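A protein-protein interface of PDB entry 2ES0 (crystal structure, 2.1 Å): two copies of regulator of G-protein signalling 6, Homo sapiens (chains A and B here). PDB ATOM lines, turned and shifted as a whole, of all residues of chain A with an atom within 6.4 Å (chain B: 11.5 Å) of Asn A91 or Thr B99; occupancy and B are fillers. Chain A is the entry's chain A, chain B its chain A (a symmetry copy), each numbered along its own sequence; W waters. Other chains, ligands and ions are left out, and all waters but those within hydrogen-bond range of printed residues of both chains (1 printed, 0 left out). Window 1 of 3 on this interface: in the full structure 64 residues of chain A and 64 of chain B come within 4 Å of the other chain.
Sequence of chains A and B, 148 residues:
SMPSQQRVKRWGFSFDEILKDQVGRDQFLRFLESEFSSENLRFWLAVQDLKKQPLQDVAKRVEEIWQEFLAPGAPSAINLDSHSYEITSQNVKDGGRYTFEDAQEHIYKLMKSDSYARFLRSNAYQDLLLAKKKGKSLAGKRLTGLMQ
The side-chain amide nitrogen of Asn A91 is in hydrogen-bond range of the backbone carbonyl oxygen of Thr B99, at 2.9 Å.
The side-chain amide oxygen of Asn A91 lies close to the backbone carbonyl oxygen of Ile A87 (3.5 Å).
O of Lys B93 sits at hydrogen-bond distance from NH2 of Arg B97 (3.3 Å).
NH2 of Arg B97 is in hydrogen-bond range of O of Asp B94.
The backbone carbonyl oxygen of Gly B96 lies within hydrogen-bond range of the side-chain hydroxyl of Thr B99 (2.6 Å).
Among the printed residues, merely in contact across the chains: Val A58 with Gly B95, Gly A95 with Val B58, Thr A88 with Phe B100, Leu A50 with Arg B97, Ile A87 with Asp B102, Thr A88 with Ala B103, Val A62 with Phe B100, Gly A95 with Leu B55, Val A58 with Arg B97, Val A58 with Gly B96, Gly A96 with Val B58, Leu A50 with Phe B100, Val A92 with Thr B99 and Val A62 with Thr B99.
Asn A91 touches one residue of chain B.
Thr B99 touches three residues of chain A.
Ile A87 touches one residue of chain B.
Thr A88 touches just these residues of chain B: Phe B100 (3.4 Å) and Ala B103 (3.5 Å).
No residue of chain B comes within 4 Å of Ser A89.
No residue of chain B comes within 4 Å of Asp A94.
Printed residues of chain B within 4 Å of Leu A50: Arg B97 (3.5 Å) and Phe B100 (3.8 Å).
Of the printed residues of chain A, Ala B103 touches Thr A88 (3.5 Å).
Printed residues of chain B within 4 Å of Gly A96: Val B58 (3.8 Å).
Of the printed residues of chain A, Asp B102 touches Ile A87.
The nearest residue of chain B that does not touch Asn A91 is Tyr B98 (4.5 Å).
The nearest residue of chain A that does not touch Thr B99 is Thr A88 (4.2 Å).
Of the 14 printed residues of chain A, 9 touch a printed residue of chain B.
Hydrophobic or aromatic side chains of chain A within 4 Å of the printed part of chain B: Leu A50, Val A58, Val A62, Ile A87 and Val A92.
Along chain A the printed residues that touch a printed residue of chain B span positions 50 to 96.
Of the 23 printed residues of chain B, 9 touch a printed residue of chain A.
Hydrophobic or aromatic side chains of chain B within 4 Å of the printed part of chain A: Leu B55, Val B58, Phe B100 and Ala B103.
Among the printed residues, 15 pairs touch across the chains.
Among the printed residues, no Asp or Glu carboxylate lies within 4 Å of a Lys or Arg side-chain nitrogen of the other chain.
Val A58 touches Gly B95, and with the chains exchanged Gly A95 touches Val B58.
Val A58 touches Gly B96, and with the chains exchanged Gly A96 touches Val B58.
9 positions are printed for both chains.
Of the 15 pairs that touch across the chains among the printed residues, 4 have their exchanged pair printed and touching as well.
Water W1 lies within hydrogen-bond range of OG1 of Thr A88 (2.6 Å), N of Ala B103 (3.1 Å), O of Thr B99 (3.3 Å) and N of Asp B102 (3.4 Å).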
ATOM      1  N   LEU A  50      32.552  15.154 -33.889  1.00  0.00           N
ATOM      2  CA  LEU A  50      31.407  15.060 -32.979  1.00  0.00           C
ATOM      3  C   LEU A  50      30.130  15.544 -33.662  1.00  0.00           C
ATOM      4  O   LEU A  50      29.083  14.919 -33.543  1.00  0.00           O
ATOM      5  CB  LEU A  50      31.673  15.867 -31.700  1.00  0.00           C
ATOM      6  CG  LEU A  50      30.503  15.990 -30.709  1.00  0.00           C
ATOM      7  CD1 LEU A  50      30.173  14.646 -30.080  1.00  0.00           C
ATOM      8  CD2 LEU A  50      30.828  17.013 -29.658  1.00  0.00           C
ATOM      9  N   VAL A  58      26.556  10.477 -29.331  1.00  0.00           N
ATOM     10  CA  VAL A  58      27.063  11.785 -28.941  1.00  0.00           C
ATOM     11  C   VAL A  58      27.561  11.815 -27.498  1.00  0.00           C
ATOM     12  O   VAL A  58      28.667  12.272 -27.239  1.00  0.00           O
ATOM     13  CB  VAL A  58      25.995  12.882 -29.162  1.00  0.00           C
ATOM     14  CG1 VAL A  58      26.394  14.186 -28.488  1.00  0.00           C
ATOM     15  CG2 VAL A  58      25.788  13.090 -30.646  1.00  0.00           C
ATOM     16  N   VAL A  62      31.288  12.857 -26.417  1.00  0.00           N
ATOM     17  CA  VAL A  62      31.536  14.034 -25.587  1.00  0.00           C
ATOM     18  C   VAL A  62      32.415  13.691 -24.375  1.00  0.00           C
ATOM     19  O   VAL A  62      33.409  14.370 -24.111  1.00  0.00           O
ATOM     20  CB  VAL A  62      30.212  14.670 -25.138  1.00  0.00           C
ATOM     21  CG1 VAL A  62      30.417  15.677 -23.977  1.00  0.00           C
ATOM     22  CG2 VAL A  62      29.543  15.335 -26.322  1.00  0.00           C
ATOM     23  N   GLU A  86      34.667  26.817 -18.199  1.00  0.00           N
ATOM     24  CA  GLU A  86      33.541  26.668 -17.288  1.00  0.00           C
ATOM     25  C   GLU A  86      32.264  26.320 -18.032  1.00  0.00           C
ATOM     26  O   GLU A  86      31.483  25.497 -17.556  1.00  0.00           O
ATOM     27  CB  GLU A  86      33.337  27.930 -16.442  1.00  0.00           C
ATOM     28  CG  GLU A  86      34.494  28.232 -15.484  1.00  0.00           C
ATOM     29  CD  GLU A  86      34.749  27.126 -14.453  1.00  0.00           C
ATOM     30  OE1 GLU A  86      33.810  26.349 -14.143  1.00  0.00           O
ATOM     31  OE2 GLU A  86      35.898  27.039 -13.947  1.00  0.00           O
ATOM     32  N   ILE A  87      32.055  26.946 -19.190  1.00  0.00           N
ATOM     33  CA  ILE A  87      30.918  26.625 -20.046  1.00  0.00           C
ATOM     34  C   ILE A  87      30.993  25.188 -20.549  1.00  0.00           C
ATOM     35  O   ILE A  87      29.997  24.470 -20.531  1.00  0.00           O
ATOM     36  CB  ILE A  87      30.808  27.594 -21.252  1.00  0.00           C
ATOM     37  CG1 ILE A  87      30.392  28.978 -20.748  1.00  0.00           C
ATOM     38  CG2 ILE A  87      29.787  27.089 -22.254  1.00  0.00           C
ATOM     39  CD1 ILE A  87      29.983  29.960 -21.839  1.00  0.00           C
ATOM     40  N   THR A  88      32.176  24.782 -21.000  1.00  0.00           N
ATOM     41  CA  THR A  88      32.375  23.427 -21.492  1.00  0.00           C
ATOM     42  C   THR A  88      32.110  22.407 -20.394  1.00  0.00           C
ATOM     43  O   THR A  88      31.438  21.413 -20.623  1.00  0.00           O
ATOM     44  CB  THR A  88      33.800  23.218 -22.020  1.00  0.00           C
ATOM     45  OG1 THR A  88      34.102  24.217 -23.003  1.00  0.00           O
ATOM     46  CG2 THR A  88      33.928  21.837 -22.641  1.00  0.00           C
ATOM     47  N   SER A  89      32.644  22.670 -19.210  1.00  0.00           N
ATOM     48  CA  SER A  89      32.500  21.771 -18.080  1.00  0.00           C
ATOM     49  C   SER A  89      31.027  21.616 -17.658  1.00  0.00           C
ATOM     50  O   SER A  89      30.570  20.521 -17.353  1.00  0.00           O
ATOM     51  CB  SER A  89      33.336  22.288 -16.911  1.00  0.00           C
ATOM     52  OG  SER A  89      33.349  21.349 -15.857  1.00  0.00           O
ATOM     53  N   GLN A  90      30.295  22.720 -17.644  1.00  0.00           N
ATOM     54  CA  GLN A  90      28.867  22.686 -17.362  1.00  0.00           C
ATOM     55  C   GLN A  90      28.088  21.884 -18.416  1.00  0.00           C
ATOM     56  O   GLN A  90      27.229  21.079 -18.071  1.00  0.00           O
ATOM     57  CB  GLN A  90      28.314  24.113 -17.290  1.00  0.00           C
ATOM     58  CG  GLN A  90      26.864  24.178 -16.854  1.00  0.00           C
ATOM     59  CD  GLN A  90      26.340  25.592 -16.776  1.00  0.00           C
ATOM     60  OE1 GLN A  90      26.150  26.249 -17.802  1.00  0.00           O
ATOM     61  NE2 GLN A  90      26.091  26.067 -15.557  1.00  0.00           N
ATOM     62  N   ASN A  91      28.392  22.115 -19.693  1.00  0.00           N
ATOM     63  CA  ASN A  91      27.739  21.401 -20.793  1.00  0.00           C
ATOM     64  C   ASN A  91      27.937  19.897 -20.670  1.00  0.00           C
ATOM     65  O   ASN A  91      26.980  19.117 -20.815  1.00  0.00           O
ATOM     66  CB  ASN A  91      28.275  21.864 -22.146  1.00  0.00           C
ATOM     67  CG  ASN A  91      27.793  23.238 -22.532  1.00  0.00           C
ATOM     68  OD1 ASN A  91      26.895  23.798 -21.896  1.00  0.00           O
ATOM     69  ND2 ASN A  91      28.384  23.795 -23.592  1.00  0.00           N
ATOM     70  N   VAL A  92      29.179  19.500 -20.387  1.00  0.00           N
ATOM     71  CA  VAL A  92      29.522  18.098 -20.235  1.00  0.00           C
ATOM     72  C   VAL A  92      28.814  17.513 -19.019  1.00  0.00           C
ATOM     73  O   VAL A  92      28.265  16.416 -19.096  1.00  0.00           O
ATOM     74  CB  VAL A  92      31.056  17.876 -20.106  1.00  0.00           C
ATOM     75  CG1 VAL A  92      31.367  16.413 -19.803  1.00  0.00           C
ATOM     76  CG2 VAL A  92      31.780  18.308 -21.366  1.00  0.00           C
ATOM     77  N   LYS A  93      28.821  18.240 -17.903  1.00  0.00           N
ATOM     78  CA  LYS A  93      28.147  17.766 -16.692  1.00  0.00           C
ATOM     79  C   LYS A  93      26.631  17.679 -16.878  1.00  0.00           C
ATOM     80  O   LYS A  93      26.038  16.661 -16.545  1.00  0.00           O
ATOM     81  CB  LYS A  93      28.477  18.641 -15.474  1.00  0.00           C
ATOM     82  CG  LYS A  93      29.563  18.073 -14.545  1.00  0.00           C
ATOM     83  CD  LYS A  93      31.001  18.530 -14.869  1.00  0.00           C
ATOM     84  CE  LYS A  93      31.830  17.444 -15.562  1.00  0.00           C
ATOM     85  NZ  LYS A  93      33.228  17.885 -15.763  1.00  0.00           N
ATOM     86  N   ASP A  94      26.026  18.753 -17.396  1.00  0.00           N
ATOM     87  CA  ASP A  94      24.589  18.814 -17.723  1.00  0.00           C
ATOM     88  C   ASP A  94      24.136  17.629 -18.577  1.00  0.00           C
ATOM     89  O   ASP A  94      23.099  17.019 -18.310  1.00  0.00           O
ATOM     90  CB  ASP A  94      24.282  20.081 -18.524  1.00  0.00           C
ATOM     91  CG  ASP A  94      24.201  21.346 -17.663  1.00  0.00           C
ATOM     92  OD1 ASP A  94      24.579  21.306 -16.478  1.00  0.00           O
ATOM     93  OD2 ASP A  94      23.746  22.391 -18.210  1.00  0.00           O
ATOM     94  N   GLY A  95      24.890  17.357 -19.642  1.00  0.00           N
ATOM     95  CA  GLY A  95      24.674  16.183 -20.479  1.00  0.00           C
ATOM     96  C   GLY A  95      23.337  16.135 -21.191  1.00  0.00           C
ATOM     97  O   GLY A  95      22.788  15.044 -21.417  1.00  0.00           O
ATOM     98  N   GLY A  96      22.825  17.307 -21.551  1.00  0.00           N
ATOM     99  CA  GLY A  96      21.543  17.430 -22.241  1.00  0.00           C
ATOM    100  C   GLY A  96      20.322  17.576 -21.346  1.00  0.00           C
ATOM    101  O   GLY A  96      19.225  17.807 -21.834  1.00  0.00           O
ATOM    102  N   GLN B  53      17.842  11.753 -14.743  1.00  0.00           N
ATOM    103  CA  GLN B  53      18.112  10.546 -15.555  1.00  0.00           C
ATOM    104  C   GLN B  53      19.587  10.219 -15.694  1.00  0.00           C
ATOM    105  O   GLN B  53      20.391  11.129 -15.860  1.00  0.00           O
ATOM    106  CB  GLN B  53      17.566  10.718 -16.979  1.00  0.00           C
ATOM    107  CG  GLN B  53      16.060  10.724 -17.083  1.00  0.00           C
ATOM    108  CD  GLN B  53      15.460   9.469 -16.533  1.00  0.00           C
ATOM    109  OE1 GLN B  53      14.762   9.494 -15.511  1.00  0.00           O
ATOM    110  NE2 GLN B  53      15.763   8.343 -17.172  1.00  0.00           N
ATOM    111  N   LEU B  55      22.944   9.495 -17.556  1.00  0.00           N
ATOM    112  CA  LEU B  55      23.425  10.093 -18.810  1.00  0.00           C
ATOM    113  C   LEU B  55      23.009   9.322 -20.068  1.00  0.00           C
ATOM    114  O   LEU B  55      22.588   9.899 -21.061  1.00  0.00           O
ATOM    115  CB  LEU B  55      24.955  10.186 -18.795  1.00  0.00           C
ATOM    116  CG  LEU B  55      25.650  11.395 -19.442  1.00  0.00           C
ATOM    117  CD1 LEU B  55      27.025  10.971 -19.985  1.00  0.00           C
ATOM    118  CD2 LEU B  55      24.841  12.060 -20.543  1.00  0.00           C
ATOM    119  N   VAL B  58      19.404  10.085 -21.419  1.00  0.00           N
ATOM    120  CA  VAL B  58      18.951  11.454 -21.628  1.00  0.00           C
ATOM    121  C   VAL B  58      18.458  11.697 -23.052  1.00  0.00           C
ATOM    122  O   VAL B  58      17.372  12.230 -23.244  1.00  0.00           O
ATOM    123  CB  VAL B  58      20.061  12.466 -21.263  1.00  0.00           C
ATOM    124  CG1 VAL B  58      19.717  13.864 -21.754  1.00  0.00           C
ATOM    125  CG2 VAL B  58      20.273  12.464 -19.765  1.00  0.00           C
ATOM    126  N   ALA B  59      19.255  11.297 -24.038  1.00  0.00           N
ATOM    127  CA  ALA B  59      18.967  11.577 -25.449  1.00  0.00           C
ATOM    128  C   ALA B  59      17.610  11.037 -25.852  1.00  0.00           C
ATOM    129  O   ALA B  59      16.845  11.713 -26.528  1.00  0.00           O
ATOM    130  CB  ALA B  59      20.045  10.983 -26.336  1.00  0.00           C
ATOM    131  N   VAL B  62      14.779  13.025 -23.972  1.00  0.00           N
ATOM    132  CA  VAL B  62      14.581  14.311 -24.634  1.00  0.00           C
ATOM    133  C   VAL B  62      13.692  14.171 -25.879  1.00  0.00           C
ATOM    134  O   VAL B  62      12.728  14.919 -26.047  1.00  0.00           O
ATOM    135  CB  VAL B  62      15.931  14.948 -24.998  1.00  0.00           C
ATOM    136  CG1 VAL B  62      15.770  16.111 -26.011  1.00  0.00           C
ATOM    137  CG2 VAL B  62      16.623  15.421 -23.737  1.00  0.00           C
ATOM    138  N   GLN B  90      16.191  23.933 -31.336  1.00  0.00           N
ATOM    139  CA  GLN B  90      17.618  23.881 -31.625  1.00  0.00           C
ATOM    140  C   GLN B  90      18.362  22.913 -30.690  1.00  0.00           C
ATOM    141  O   GLN B  90      19.188  22.127 -31.143  1.00  0.00           O
ATOM    142  CB  GLN B  90      18.227  25.281 -31.505  1.00  0.00           C
ATOM    143  CG  GLN B  90      19.681  25.346 -31.932  1.00  0.00           C
ATOM    144  CD  GLN B  90      20.262  26.735 -31.819  1.00  0.00           C
ATOM    145  OE1 GLN B  90      20.475  27.239 -30.716  1.00  0.00           O
ATOM    146  NE2 GLN B  90      20.533  27.359 -32.964  1.00  0.00           N
ATOM    147  N   ASN B  91      18.064  22.981 -29.392  1.00  0.00           N
ATOM    148  CA  ASN B  91      18.684  22.100 -28.401  1.00  0.00           C
ATOM    149  C   ASN B  91      18.426  20.635 -28.726  1.00  0.00           C
ATOM    150  O   ASN B  91      19.351  19.805 -28.689  1.00  0.00           O
ATOM    151  CB  ASN B  91      18.163  22.397 -26.996  1.00  0.00           C
ATOM    152  CG  ASN B  91      18.699  23.686 -26.430  1.00  0.00           C
ATOM    153  OD1 ASN B  91      19.621  24.290 -26.987  1.00  0.00           O
ATOM    154  ND2 ASN B  91      18.128  24.118 -25.303  1.00  0.00           N
ATOM    155  N   VAL B  92      17.170  20.331 -29.056  1.00  0.00           N
ATOM    156  CA  VAL B  92      16.772  18.977 -29.395  1.00  0.00           C
ATOM    157  C   VAL B  92      17.459  18.533 -30.680  1.00  0.00           C
ATOM    158  O   VAL B  92      17.963  17.415 -30.754  1.00  0.00           O
ATOM    159  CB  VAL B  92      15.230  18.836 -29.548  1.00  0.00           C
ATOM    160  CG1 VAL B  92      14.861  17.441 -30.046  1.00  0.00           C
ATOM    161  CG2 VAL B  92      14.520  19.123 -28.239  1.00  0.00           C
ATOM    162  N   LYS B  93      17.483  19.404 -31.688  1.00  0.00           N
ATOM    163  CA  LYS B  93      18.141  19.072 -32.954  1.00  0.00           C
ATOM    164  C   LYS B  93      19.652  18.899 -32.785  1.00  0.00           C
ATOM    165  O   LYS B  93      20.205  17.911 -33.255  1.00  0.00           O
ATOM    166  CB  LYS B  93      17.851  20.114 -34.042  1.00  0.00           C
ATOM    167  CG  LYS B  93      16.745  19.722 -35.037  1.00  0.00           C
ATOM    168  CD  LYS B  93      15.326  20.188 -34.650  1.00  0.00           C
ATOM    169  CE  LYS B  93      14.452  19.053 -34.107  1.00  0.00           C
ATOM    170  NZ  LYS B  93      13.072  19.517 -33.845  1.00  0.00           N
ATOM    171  N   ASP B  94      20.299  19.868 -32.129  1.00  0.00           N
ATOM    172  CA  ASP B  94      21.736  19.826 -31.801  1.00  0.00           C
ATOM    173  C   ASP B  94      22.139  18.519 -31.116  1.00  0.00           C
ATOM    174  O   ASP B  94      23.151  17.910 -31.465  1.00  0.00           O
ATOM    175  CB  ASP B  94      22.091  20.960 -30.837  1.00  0.00           C
ATOM    176  CG  ASP B  94      22.226  22.325 -31.519  1.00  0.00           C
ATOM    177  OD1 ASP B  94      21.850  22.460 -32.698  1.00  0.00           O
ATOM    178  OD2 ASP B  94      22.721  23.269 -30.838  1.00  0.00           O
ATOM    179  N   GLY B  95      21.372  18.136 -30.095  1.00  0.00           N
ATOM    180  CA  GLY B  95      21.538  16.853 -29.424  1.00  0.00           C
ATOM    181  C   GLY B  95      22.869  16.656 -28.729  1.00  0.00           C
ATOM    182  O   GLY B  95      23.374  15.523 -28.655  1.00  0.00           O
ATOM    183  N   GLY B  96      23.428  17.747 -28.216  1.00  0.00           N
ATOM    184  CA  GLY B  96      24.711  17.724 -27.519  1.00  0.00           C
ATOM    185  C   GLY B  96      25.940  17.940 -28.389  1.00  0.00           C
ATOM    186  O   GLY B  96      27.044  18.059 -27.878  1.00  0.00           O
ATOM    187  N   ARG B  97      25.748  18.025 -29.700  1.00  0.00           N
ATOM    188  CA  ARG B  97      26.871  18.079 -30.649  1.00  0.00           C
ATOM    189  C   ARG B  97      27.688  19.376 -30.585  1.00  0.00           C
ATOM    190  O   ARG B  97      28.791  19.438 -31.128  1.00  0.00           O
ATOM    191  CB  ARG B  97      26.368  17.858 -32.066  1.00  0.00           C
ATOM    192  CG  ARG B  97      25.890  16.450 -32.333  1.00  0.00           C
ATOM    193  CD  ARG B  97      25.348  16.349 -33.735  1.00  0.00           C
ATOM    194  NE  ARG B  97      24.719  15.058 -34.026  1.00  0.00           N
ATOM    195  CZ  ARG B  97      23.441  14.758 -33.766  1.00  0.00           C
ATOM    196  NH1 ARG B  97      22.955  13.558 -34.078  1.00  0.00           N
ATOM    197  NH2 ARG B  97      22.633  15.650 -33.205  1.00  0.00           N
ATOM    198  N   TYR B  98      27.156  20.395 -29.908  1.00  0.00           N
ATOM    199  CA  TYR B  98      27.810  21.706 -29.820  1.00  0.00           C
ATOM    200  C   TYR B  98      28.230  22.037 -28.392  1.00  0.00           C
ATOM    201  O   TYR B  98      28.397  23.195 -28.027  1.00  0.00           O
ATOM    202  CB  TYR B  98      26.914  22.765 -30.479  1.00  0.00           C
ATOM    203  CG  TYR B  98      26.771  22.445 -31.946  1.00  0.00           C
ATOM    204  CD1 TYR B  98      27.623  23.015 -32.884  1.00  0.00           C
ATOM    205  CD2 TYR B  98      25.853  21.494 -32.386  1.00  0.00           C
ATOM    206  CE1 TYR B  98      27.541  22.683 -34.219  1.00  0.00           C
ATOM    207  CE2 TYR B  98      25.762  21.151 -33.719  1.00  0.00           C
ATOM    208  CZ  TYR B  98      26.608  21.751 -34.635  1.00  0.00           C
ATOM    209  OH  TYR B  98      26.532  21.422 -35.963  1.00  0.00           O
ATOM    210  N   THR B  99      28.430  20.972 -27.609  1.00  0.00           N
ATOM    211  CA  THR B  99      28.950  21.020 -26.258  1.00  0.00           C
ATOM    212  C   THR B  99      30.269  21.809 -26.152  1.00  0.00           C
ATOM    213  O   THR B  99      30.495  22.485 -25.142  1.00  0.00           O
ATOM    214  CB  THR B  99      29.162  19.564 -25.737  1.00  0.00           C
ATOM    215  OG1 THR B  99      27.893  18.904 -25.591  1.00  0.00           O
ATOM    216  CG2 THR B  99      29.889  19.523 -24.410  1.00  0.00           C
ATOM    217  N   PHE B 100      31.113  21.728 -27.191  1.00  0.00           N
ATOM    218  CA  PHE B 100      32.460  22.342 -27.185  1.00  0.00           C
ATOM    219  C   PHE B 100      32.576  23.593 -28.076  1.00  0.00           C
ATOM    220  O   PHE B 100      33.665  23.908 -28.554  1.00  0.00           O
ATOM    221  CB  PHE B 100      33.504  21.304 -27.629  1.00  0.00           C
ATOM    222  CG  PHE B 100      33.552  20.076 -26.757  1.00  0.00           C
ATOM    223  CD1 PHE B 100      34.189  20.112 -25.528  1.00  0.00           C
ATOM    224  CD2 PHE B 100      32.962  18.896 -27.165  1.00  0.00           C
ATOM    225  CE1 PHE B 100      34.234  18.978 -24.711  1.00  0.00           C
ATOM    226  CE2 PHE B 100      33.000  17.755 -26.356  1.00  0.00           C
ATOM    227  CZ  PHE B 100      33.645  17.795 -25.132  1.00  0.00           C
ATOM    228  N   GLU B 101      31.465  24.297 -28.293  1.00  0.00           N
ATOM    229  CA  GLU B 101      31.412  25.437 -29.232  1.00  0.00           C
ATOM    230  C   GLU B 101      32.382  26.564 -28.900  1.00  0.00           C
ATOM    231  O   GLU B 101      33.129  27.032 -29.768  1.00  0.00           O
ATOM    232  CB  GLU B 101      29.989  26.012 -29.291  1.00  0.00           C
ATOM    233  CG  GLU B 101      29.765  27.080 -30.369  1.00  0.00           C
ATOM    234  CD  GLU B 101      28.281  27.457 -30.551  1.00  0.00           C
ATOM    235  OE1 GLU B 101      27.438  27.074 -29.686  1.00  0.00           O
ATOM    236  N   ASP B 102      32.344  27.032 -27.658  1.00  0.00           N
ATOM    237  CA  ASP B 102      33.222  28.129 -27.225  1.00  0.00           C
ATOM    238  C   ASP B 102      34.678  27.666 -27.179  1.00  0.00           C
ATOM    239  O   ASP B 102      35.565  28.346 -27.672  1.00  0.00           O
ATOM    240  CB  ASP B 102      32.793  28.674 -25.862  1.00  0.00           C
ATOM    241  CG  ASP B 102      31.408  29.293 -25.898  1.00  0.00           C
ATOM    242  OD1 ASP B 102      31.232  30.333 -26.582  1.00  0.00           O
ATOM    243  OD2 ASP B 102      30.494  28.723 -25.266  1.00  0.00           O
ATOM    244  N   ALA B 103      34.895  26.490 -26.611  1.00  0.00           N
ATOM    245  CA  ALA B 103      36.213  25.869 -26.568  1.00  0.00           C
ATOM    246  C   ALA B 103      36.825  25.730 -27.958  1.00  0.00           C
ATOM    247  O   ALA B 103      37.966  26.119 -28.172  1.00  0.00           O
ATOM    248  CB  ALA B 103      36.129  24.519 -25.890  1.00  0.00           C
ATOM    249  N   GLN B 104      36.070  25.184 -28.902  1.00  0.00           N
ATOM    250  CA  GLN B 104      36.585  25.005 -30.257  1.00  0.00           C
ATOM    251  C   GLN B 104      36.939  26.339 -30.920  1.00  0.00           C
ATOM    252  O   GLN B 104      37.913  26.426 -31.663  1.00  0.00           O
ATOM    253  CB  GLN B 104      35.588  24.256 -31.132  1.00  0.00           C
ATOM    254  CG  GLN B 104      36.140  23.907 -32.523  1.00  0.00           C
ATOM    255  CD  GLN B 104      35.140  23.194 -33.402  1.00  0.00           C
ATOM    256  OE1 GLN B 104      33.918  23.360 -33.247  1.00  0.00           O
ATOM    257  NE2 GLN B 104      35.648  22.398 -34.353  1.00  0.00           N
ATOM    258  N   GLU B 105      36.123  27.359 -30.673  1.00  0.00           N
ATOM    259  CA  GLU B 105      36.347  28.685 -31.250  1.00  0.00           C
ATOM    260  C   GLU B 105      37.626  29.314 -30.684  1.00  0.00           C
ATOM    261  O   GLU B 105      38.402  29.929 -31.415  1.00  0.00           O
ATOM    262  CB  GLU B 105      35.121  29.580 -30.996  1.00  0.00           C
ATOM    263  CG  GLU B 105      35.232  31.021 -31.505  1.00  0.00           C
ATOM    264  CD  GLU B 105      35.460  31.129 -33.015  1.00  0.00           C
ATOM    265  OE1 GLU B 105      35.127  30.160 -33.753  1.00  0.00           O
ATOM    266  OE2 GLU B 105      35.958  32.198 -33.469  1.00  0.00           O
ATOM    267  N   HIS B 106      37.840  29.152 -29.382  1.00  0.00           N
ATOM    268  CA  HIS B 106      39.060  29.644 -28.740  1.00  0.00           C
ATOM    269  C   HIS B 106      40.289  28.981 -29.370  1.00  0.00           C
ATOM    270  O   HIS B 106      41.242  29.657 -29.751  1.00  0.00           O
ATOM    271  CB  HIS B 106      39.010  29.383 -27.232  1.00  0.00           C
ATOM    272  CG  HIS B 106      40.207  29.889 -26.487  1.00  0.00           C
ATOM    273  ND1 HIS B 106      41.261  29.071 -26.139  1.00  0.00           N
ATOM    274  CD2 HIS B 106      40.524  31.126 -26.036  1.00  0.00           C
ATOM    275  CE1 HIS B 106      42.173  29.782 -25.502  1.00  0.00           C
ATOM    276  NE2 HIS B 106      41.751  31.033 -25.423  1.00  0.00           N
ATOM    277  N   ILE B 107      40.235  27.658 -29.525  1.00  0.00           N
ATOM    278  CA  ILE B 107      41.346  26.894 -30.096  1.00  0.00           C
ATOM    279  C   ILE B 107      41.543  27.179 -31.590  1.00  0.00           C
ATOM    280  O   ILE B 107      42.681  27.254 -32.068  1.00  0.00           O
ATOM    281  CB  ILE B 107      41.149  25.375 -29.857  1.00  0.00           C
ATOM    282  CG1 ILE B 107      41.134  25.060 -28.348  1.00  0.00           C
ATOM    283  CG2 ILE B 107      42.204  24.552 -30.582  1.00  0.00           C
ATOM    284  CD1 ILE B 107      42.391  25.432 -27.597  1.00  0.00           C
HETATM  285  O   HOH W   1      32.719  24.889 -25.038  1.00  0.00           O
